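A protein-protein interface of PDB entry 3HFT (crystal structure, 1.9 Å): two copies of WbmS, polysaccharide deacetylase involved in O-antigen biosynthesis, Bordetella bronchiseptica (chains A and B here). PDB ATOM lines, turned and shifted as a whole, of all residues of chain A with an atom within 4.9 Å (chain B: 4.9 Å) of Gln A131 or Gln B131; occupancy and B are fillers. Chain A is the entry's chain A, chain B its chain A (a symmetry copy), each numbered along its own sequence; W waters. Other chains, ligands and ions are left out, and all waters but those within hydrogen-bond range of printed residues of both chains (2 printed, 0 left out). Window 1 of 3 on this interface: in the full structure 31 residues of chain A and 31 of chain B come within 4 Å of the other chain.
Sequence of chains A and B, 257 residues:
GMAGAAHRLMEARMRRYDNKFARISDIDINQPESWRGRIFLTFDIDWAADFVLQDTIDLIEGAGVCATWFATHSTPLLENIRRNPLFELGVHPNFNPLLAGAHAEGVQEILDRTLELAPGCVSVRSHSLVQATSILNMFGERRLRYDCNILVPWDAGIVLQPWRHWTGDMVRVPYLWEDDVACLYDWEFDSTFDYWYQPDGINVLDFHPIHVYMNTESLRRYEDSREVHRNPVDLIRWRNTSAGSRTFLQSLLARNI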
ATOM      1  N   LEU A 129     -31.512   7.436  -4.185  1.00  0.00           N
ATOM      2  CA  LEU A 129     -30.312   7.115  -4.957  1.00  0.00           C
ATOM      3  C   LEU A 129     -29.307   6.356  -4.124  1.00  0.00           C
ATOM      4  O   LEU A 129     -28.088   6.539  -4.242  1.00  0.00           O
ATOM      5  CB  LEU A 129     -29.730   8.414  -5.559  1.00  0.00           C
ATOM      6  CG  LEU A 129     -30.686   9.204  -6.471  1.00  0.00           C
ATOM      7  CD1 LEU A 129     -29.986  10.386  -7.159  1.00  0.00           C
ATOM      8  CD2 LEU A 129     -31.337   8.299  -7.529  1.00  0.00           C
ATOM      9  N   VAL A 130     -29.829   5.478  -3.265  1.00  0.00           N
ATOM     10  CA  VAL A 130     -28.974   4.624  -2.472  1.00  0.00           C
ATOM     11  C   VAL A 130     -28.329   3.589  -3.401  1.00  0.00           C
ATOM     12  O   VAL A 130     -29.016   2.823  -4.092  1.00  0.00           O
ATOM     13  CB  VAL A 130     -29.727   3.894  -1.312  1.00  0.00           C
ATOM     14  CG1 VAL A 130     -28.714   3.013  -0.524  1.00  0.00           C
ATOM     15  CG2 VAL A 130     -30.474   4.859  -0.369  1.00  0.00           C
ATOM     16  N   GLN A 131     -27.002   3.545  -3.414  1.00  0.00           N
ATOM     17  CA  GLN A 131     -26.270   2.649  -4.312  1.00  0.00           C
ATOM     18  C   GLN A 131     -24.923   2.312  -3.692  1.00  0.00           C
ATOM     19  O   GLN A 131     -24.472   2.993  -2.748  1.00  0.00           O
ATOM     20  CB  GLN A 131     -26.099   3.318  -5.673  1.00  0.00           C
ATOM     21  CG  GLN A 131     -25.407   4.661  -5.594  1.00  0.00           C
ATOM     22  CD  GLN A 131     -25.651   5.525  -6.817  1.00  0.00           C
ATOM     23  OE1 GLN A 131     -25.008   5.337  -7.854  1.00  0.00           O
ATOM     24  NE2 GLN A 131     -26.576   6.498  -6.691  1.00  0.00           N
ATOM     25  N   ALA A 132     -24.330   1.217  -4.186  1.00  0.00           N
ATOM     26  CA  ALA A 132     -23.060   0.714  -3.719  1.00  0.00           C
ATOM     27  C   ALA A 132     -22.673  -0.383  -4.712  1.00  0.00           C
ATOM     28  O   ALA A 132     -23.526  -0.950  -5.406  1.00  0.00           O
ATOM     29  CB  ALA A 132     -23.215   0.065  -2.284  1.00  0.00           C
ATOM     30  N   THR A 133     -21.401  -0.720  -4.741  1.00  0.00           N
ATOM     31  CA  THR A 133     -20.970  -1.835  -5.557  1.00  0.00           C
ATOM     32  C   THR A 133     -21.752  -3.116  -5.245  1.00  0.00           C
ATOM     33  O   THR A 133     -22.143  -3.827  -6.177  1.00  0.00           O
ATOM     34  CB  THR A 133     -19.468  -2.019  -5.457  1.00  0.00           C
ATOM     35  OG1 THR A 133     -18.836  -0.839  -6.019  1.00  0.00           O
ATOM     36  CG2 THR A 133     -19.002  -3.294  -6.231  1.00  0.00           C
ATOM     37  N   ILE A 135     -24.730  -3.408  -3.970  1.00  0.00           N
ATOM     38  CA  ILE A 135     -26.120  -3.192  -4.391  1.00  0.00           C
ATOM     39  C   ILE A 135     -26.238  -3.463  -5.900  1.00  0.00           C
ATOM     40  O   ILE A 135     -27.108  -4.224  -6.326  1.00  0.00           O
ATOM     41  CB  ILE A 135     -26.644  -1.796  -4.009  1.00  0.00           C
ATOM     42  CG1 ILE A 135     -26.756  -1.683  -2.477  1.00  0.00           C
ATOM     43  CG2 ILE A 135     -27.997  -1.525  -4.672  1.00  0.00           C
ATOM     44  CD1 ILE A 135     -27.153  -0.285  -1.973  1.00  0.00           C
ATOM     45  N   LEU A 136     -25.357  -2.869  -6.701  1.00  0.00           N
ATOM     46  CA  LEU A 136     -25.369  -3.118  -8.151  1.00  0.00           C
ATOM     47  C   LEU A 136     -25.101  -4.598  -8.449  1.00  0.00           C
ATOM     48  O   LEU A 136     -25.706  -5.141  -9.350  1.00  0.00           O
ATOM     49  CB  LEU A 136     -24.383  -2.240  -8.896  1.00  0.00           C
ATOM     50  CG  LEU A 136     -24.970  -0.910  -9.410  1.00  0.00           C
ATOM     51  CD1 LEU A 136     -25.593  -0.101  -8.285  1.00  0.00           C
ATOM     52  CD2 LEU A 136     -23.907  -0.129 -10.151  1.00  0.00           C
ATOM     53  N   ASN A 149     -29.364   5.186 -11.269  1.00  0.00           N
ATOM     54  CA  ASN A 149     -29.032   5.857  -9.992  1.00  0.00           C
ATOM     55  C   ASN A 149     -28.028   7.023 -10.022  1.00  0.00           C
ATOM     56  O   ASN A 149     -27.848   7.694  -9.021  1.00  0.00           O
ATOM     57  CB  ASN A 149     -28.510   4.798  -9.017  1.00  0.00           C
ATOM     58  CG  ASN A 149     -29.646   4.017  -8.370  1.00  0.00           C
ATOM     59  OD1 ASN A 149     -30.554   4.618  -7.844  1.00  0.00           O
ATOM     60  ND2 ASN A 149     -29.567   2.702  -8.369  1.00  0.00           N
ATOM     61  N   ILE A 150     -27.376   7.251 -11.159  1.00  0.00           N
ATOM     62  CA  ILE A 150     -26.401   8.359 -11.303  1.00  0.00           C
ATOM     63  C   ILE A 150     -27.093   9.605 -11.858  1.00  0.00           C
ATOM     64  O   ILE A 150     -27.640   9.580 -12.980  1.00  0.00           O
ATOM     65  CB  ILE A 150     -25.257   8.012 -12.286  1.00  0.00           C
ATOM     66  CG1 ILE A 150     -24.401   6.828 -11.780  1.00  0.00           C
ATOM     67  CG2 ILE A 150     -24.300   9.247 -12.495  1.00  0.00           C
ATOM     68  CD1 ILE A 150     -23.555   7.147 -10.637  1.00  0.00           C
ATOM     69  N   ARG A 172     -25.303   1.349 -16.964  1.00  0.00           N
ATOM     70  CA  ARG A 172     -25.602   2.481 -16.118  1.00  0.00           C
ATOM     71  C   ARG A 172     -26.127   3.605 -17.001  1.00  0.00           C
ATOM     72  O   ARG A 172     -25.523   3.978 -18.022  1.00  0.00           O
ATOM     73  CB  ARG A 172     -24.376   2.925 -15.328  1.00  0.00           C
ATOM     74  CG  ARG A 172     -23.799   1.824 -14.490  1.00  0.00           C
ATOM     75  CD  ARG A 172     -23.146   2.425 -13.285  1.00  0.00           C
ATOM     76  NE  ARG A 172     -24.150   2.818 -12.310  1.00  0.00           N
ATOM     77  CZ  ARG A 172     -23.875   3.253 -11.095  1.00  0.00           C
ATOM     78  NH1 ARG A 172     -22.616   3.377 -10.716  1.00  0.00           N
ATOM     79  NH2 ARG A 172     -24.849   3.555 -10.255  1.00  0.00           N
ATOM     80  N   LEU B 129     -18.163   2.525  -2.567  1.00  0.00           N
ATOM     81  CA  LEU B 129     -18.913   3.604  -3.209  1.00  0.00           C
ATOM     82  C   LEU B 129     -20.339   3.653  -2.717  1.00  0.00           C
ATOM     83  O   LEU B 129     -21.281   3.937  -3.469  1.00  0.00           O
ATOM     84  CB  LEU B 129     -18.814   3.451  -4.743  1.00  0.00           C
ATOM     85  CG  LEU B 129     -17.385   3.457  -5.316  1.00  0.00           C
ATOM     86  CD1 LEU B 129     -17.377   3.467  -6.853  1.00  0.00           C
ATOM     87  CD2 LEU B 129     -16.567   4.644  -4.785  1.00  0.00           C
ATOM     88  N   VAL B 130     -20.504   3.376  -1.421  1.00  0.00           N
ATOM     89  CA  VAL B 130     -21.807   3.475  -0.806  1.00  0.00           C
ATOM     90  C   VAL B 130     -22.187   4.957  -0.711  1.00  0.00           C
ATOM     91  O   VAL B 130     -21.471   5.771  -0.109  1.00  0.00           O
ATOM     92  CB  VAL B 130     -21.876   2.822   0.613  1.00  0.00           C
ATOM     93  CG1 VAL B 130     -23.319   2.979   1.176  1.00  0.00           C
ATOM     94  CG2 VAL B 130     -21.433   1.345   0.626  1.00  0.00           C
ATOM     95  N   GLN B 131     -23.325   5.319  -1.292  1.00  0.00           N
ATOM     96  CA  GLN B 131     -23.759   6.718  -1.331  1.00  0.00           C
ATOM     97  C   GLN B 131     -25.275   6.768  -1.415  1.00  0.00           C
ATOM     98  O   GLN B 131     -25.926   5.751  -1.733  1.00  0.00           O
ATOM     99  CB  GLN B 131     -23.116   7.418  -2.525  1.00  0.00           C
ATOM    100  CG  GLN B 131     -23.412   6.741  -3.844  1.00  0.00           C
ATOM    101  CD  GLN B 131     -22.431   7.119  -4.937  1.00  0.00           C
ATOM    102  OE1 GLN B 131     -22.551   8.187  -5.543  1.00  0.00           O
ATOM    103  NE2 GLN B 131     -21.460   6.224  -5.209  1.00  0.00           N
ATOM    104  N   ALA B 132     -25.825   7.937  -1.059  1.00  0.00           N
ATOM    105  CA  ALA B 132     -27.247   8.183  -1.048  1.00  0.00           C
ATOM    106  C   ALA B 132     -27.392   9.688  -0.816  1.00  0.00           C
ATOM    107  O   ALA B 132     -26.485  10.347  -0.292  1.00  0.00           O
ATOM    108  CB  ALA B 132     -27.932   7.418   0.155  1.00  0.00           C
ATOM    109  N   THR B 133     -28.548  10.221  -1.151  1.00  0.00           N
ATOM    110  CA  THR B 133     -28.816  11.610  -0.847  1.00  0.00           C
ATOM    111  C   THR B 133     -28.606  11.927   0.638  1.00  0.00           C
ATOM    112  O   THR B 133     -28.019  12.968   0.956  1.00  0.00           O
ATOM    113  CB  THR B 133     -30.189  12.010  -1.350  1.00  0.00           C
ATOM    114  OG1 THR B 133     -30.181  11.908  -2.798  1.00  0.00           O
ATOM    115  CG2 THR B 133     -30.546  13.469  -0.920  1.00  0.00           C
ATOM    116  N   ILE B 135     -26.720  10.382   2.790  1.00  0.00           N
ATOM    117  CA  ILE B 135     -25.287  10.239   3.075  1.00  0.00           C
ATOM    118  C   ILE B 135     -24.560  11.534   2.675  1.00  0.00           C
ATOM    119  O   ILE B 135     -23.809  12.095   3.474  1.00  0.00           O
ATOM    120  CB  ILE B 135     -24.671   8.997   2.405  1.00  0.00           C
ATOM    121  CG1 ILE B 135     -25.250   7.720   3.044  1.00  0.00           C
ATOM    122  CG2 ILE B 135     -23.145   9.017   2.525  1.00  0.00           C
ATOM    123  CD1 ILE B 135     -24.798   6.415   2.369  1.00  0.00           C
ATOM    124  N   LEU B 136     -24.799  12.021   1.459  1.00  0.00           N
ATOM    125  CA  LEU B 136     -24.185  13.283   1.019  1.00  0.00           C
ATOM    126  C   LEU B 136     -24.641  14.447   1.908  1.00  0.00           C
ATOM    127  O   LEU B 136     -23.845  15.312   2.208  1.00  0.00           O
ATOM    128  CB  LEU B 136     -24.470  13.586  -0.438  1.00  0.00           C
ATOM    129  CG  LEU B 136     -23.405  13.059  -1.422  1.00  0.00           C
ATOM    130  CD1 LEU B 136     -23.191  11.563  -1.266  1.00  0.00           C
ATOM    131  CD2 LEU B 136     -23.782  13.435  -2.839  1.00  0.00           C
ATOM    132  N   ASN B 149     -17.302   9.841  -4.932  1.00  0.00           N
ATOM    133  CA  ASN B 149     -18.006   8.543  -5.040  1.00  0.00           C
ATOM    134  C   ASN B 149     -18.563   8.130  -6.415  1.00  0.00           C
ATOM    135  O   ASN B 149     -19.011   7.009  -6.574  1.00  0.00           O
ATOM    136  CB  ASN B 149     -19.160   8.540  -4.033  1.00  0.00           C
ATOM    137  CG  ASN B 149     -18.678   8.219  -2.624  1.00  0.00           C
ATOM    138  OD1 ASN B 149     -17.996   7.237  -2.440  1.00  0.00           O
ATOM    139  ND2 ASN B 149     -19.069   9.009  -1.645  1.00  0.00           N
ATOM    140  N   ILE B 150     -18.542   9.035  -7.389  1.00  0.00           N
ATOM    141  CA  ILE B 150     -19.036   8.737  -8.755  1.00  0.00           C
ATOM    142  C   ILE B 150     -17.884   8.264  -9.644  1.00  0.00           C
ATOM    143  O   ILE B 150     -16.909   9.011  -9.867  1.00  0.00           O
ATOM    144  CB  ILE B 150     -19.648   9.980  -9.444  1.00  0.00           C
ATOM    145  CG1 ILE B 150     -20.901  10.494  -8.701  1.00  0.00           C
ATOM    146  CG2 ILE B 150     -20.066   9.653 -10.929  1.00  0.00           C
ATOM    147  CD1 ILE B 150     -22.070   9.633  -8.832  1.00  0.00           C
ATOM    148  N   ARG B 172     -19.102  17.485  -6.338  1.00  0.00           N
ATOM    149  CA  ARG B 172     -18.956  16.096  -6.703  1.00  0.00           C
ATOM    150  C   ARG B 172     -17.826  15.990  -7.718  1.00  0.00           C
ATOM    151  O   ARG B 172     -17.782  16.707  -8.732  1.00  0.00           O
ATOM    152  CB  ARG B 172     -20.256  15.526  -7.259  1.00  0.00           C
ATOM    153  CG  ARG B 172     -21.403  15.667  -6.305  1.00  0.00           C
ATOM    154  CD  ARG B 172     -22.366  14.545  -6.539  1.00  0.00           C
ATOM    155  NE  ARG B 172     -21.859  13.315  -5.953  1.00  0.00           N
ATOM    156  CZ  ARG B 172     -22.544  12.190  -5.880  1.00  0.00           C
ATOM    157  NH1 ARG B 172     -23.763  12.134  -6.386  1.00  0.00           N
ATOM    158  NH2 ARG B 172     -22.024  11.125  -5.297  1.00  0.00           N
HETATM  159  O   HOH W   1     -26.541   9.030  -4.076  1.00  0.00           O
HETATM  160  O   HOH W   2     -22.066   2.729  -6.029  1.00  0.00           O
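Leu A129 touches Ala B132.
Val A130 touches Gln B131 (CA to O, 3.3 Å).
Val A130 touches Ala B132.
Val B130 touches Gln A131 (CA to O, 3.3 Å).
O of Leu B129 touches CA of Ala A132, at 3.7 Å.
Ala A132 touches Val B130.
CD1 of Ile B150 touches CD1 of Ile A150, at 3.4 Å.
Gln A131 touches three residues of chain B.
Thr A133 touches none of the printed residues of chain B.
Of the printed residues of chain B, Ile A150 touches Ile B150 (3.4 Å).
Printed residues of chain A within 4 Å of Leu B129: Gln A131 and Ala A132.
Of the printed residues of chain A, Val B130 touches Gln A131 (3.3 Å) and Ala A132 (3.6 Å).
Of chain A, only Leu A129, Val A130 and Gln A131 come within 4 Å of Gln B131.
Of the printed residues of chain A, Ala B132 touches Leu A129 and Val A130.
Printed residues of chain A within 4 Å of Ile B150: Ile A150 (3.4 Å).
The nearest printed residue of chain B that does not touch Gln A131 is Ala B132 (5.1 Å).
The nearest printed residue of chain A that does not touch Gln B131 is Ala A132 (5.1 Å).
The nearest printed residue of chain B that does not touch Ile A150 is Gln B131 (5.3 Å).
Hydrophobic or aromatic side chains of chain B within 4 Å of the printed part of chain A: Val B130, Ala B132 and Ile B150.
Printed residues of chain A that touch a printed residue of chain B: Leu A129, Val A130, Gln A131, Ala A132 and Ile A150.
Hydrophobic or aromatic side chains of chain A that line the printed part of chain B: Val A130, Ala A132 and Ile A150.
Among the printed residues, 10 pairs touch across the chains.
Water W2 lies within hydrogen-bond range of the backbone carbonyl oxygen of Leu B129 (2.9 Å) and the backbone NH of Ala A132 (3.3 Å).
Water W1 bridges O of Leu A129 (2.9 Å) and N of Ala B132 (3.3 Å).
The backbone carbonyl oxygen (O) of Leu B129 lies close to the backbone carbonyl oxygen (O) of Gln A131 (3.4 Å).
O of Gln B131 lies close to O of Leu A129 (3.4 Å).
O of Gln B131 sits at hydrogen-bond distance from N of Gln A131 (3.0 Å).
Leu A129 touches Gln B131, and with the chains exchanged Gln A131 touches Leu B129.
Leu A129 touches Ala B132, and with the chains exchanged Ala A132 touches Leu B129.
Val A130 touches Ala B132, and with the chains exchanged Ala A132 touches Val B130.
Ile A150 touches its own counterpart, Ile B150.
Positions printed for both chains: 129, 130, 131, 132, 133, 135, 136, 149, 150 and 172.
Of the 10 pairs that touch across the chains among the printed residues, 10 have their exchanged pair printed and touching as well.
O of Leu A129 lies within hydrogen-bond range of NE2 of Gln A131.
NE2 of Gln A131 is in hydrogen-bond range of O of Asn A149, at 2.9 Å.
The side-chain amide nitrogen of Gln B131 lies within hydrogen-bond range of the backbone carbonyl oxygen of Asn B149, 2.9 Å away.
NH2 of Arg B172 is in hydrogen-bond range of OE1 of Gln B131 (3.0 Å).
The backbone carbonyl oxygen (O) of Leu B129 lies within hydrogen-bond range of the side-chain amide nitrogen (NE2) of Gln B131, 2.9 Å away.
The guanidinium group (NH2) of Arg A172 lies within hydrogen-bond range of the side-chain amide oxygen (OE1) of Gln A131, at 3.0 Å.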
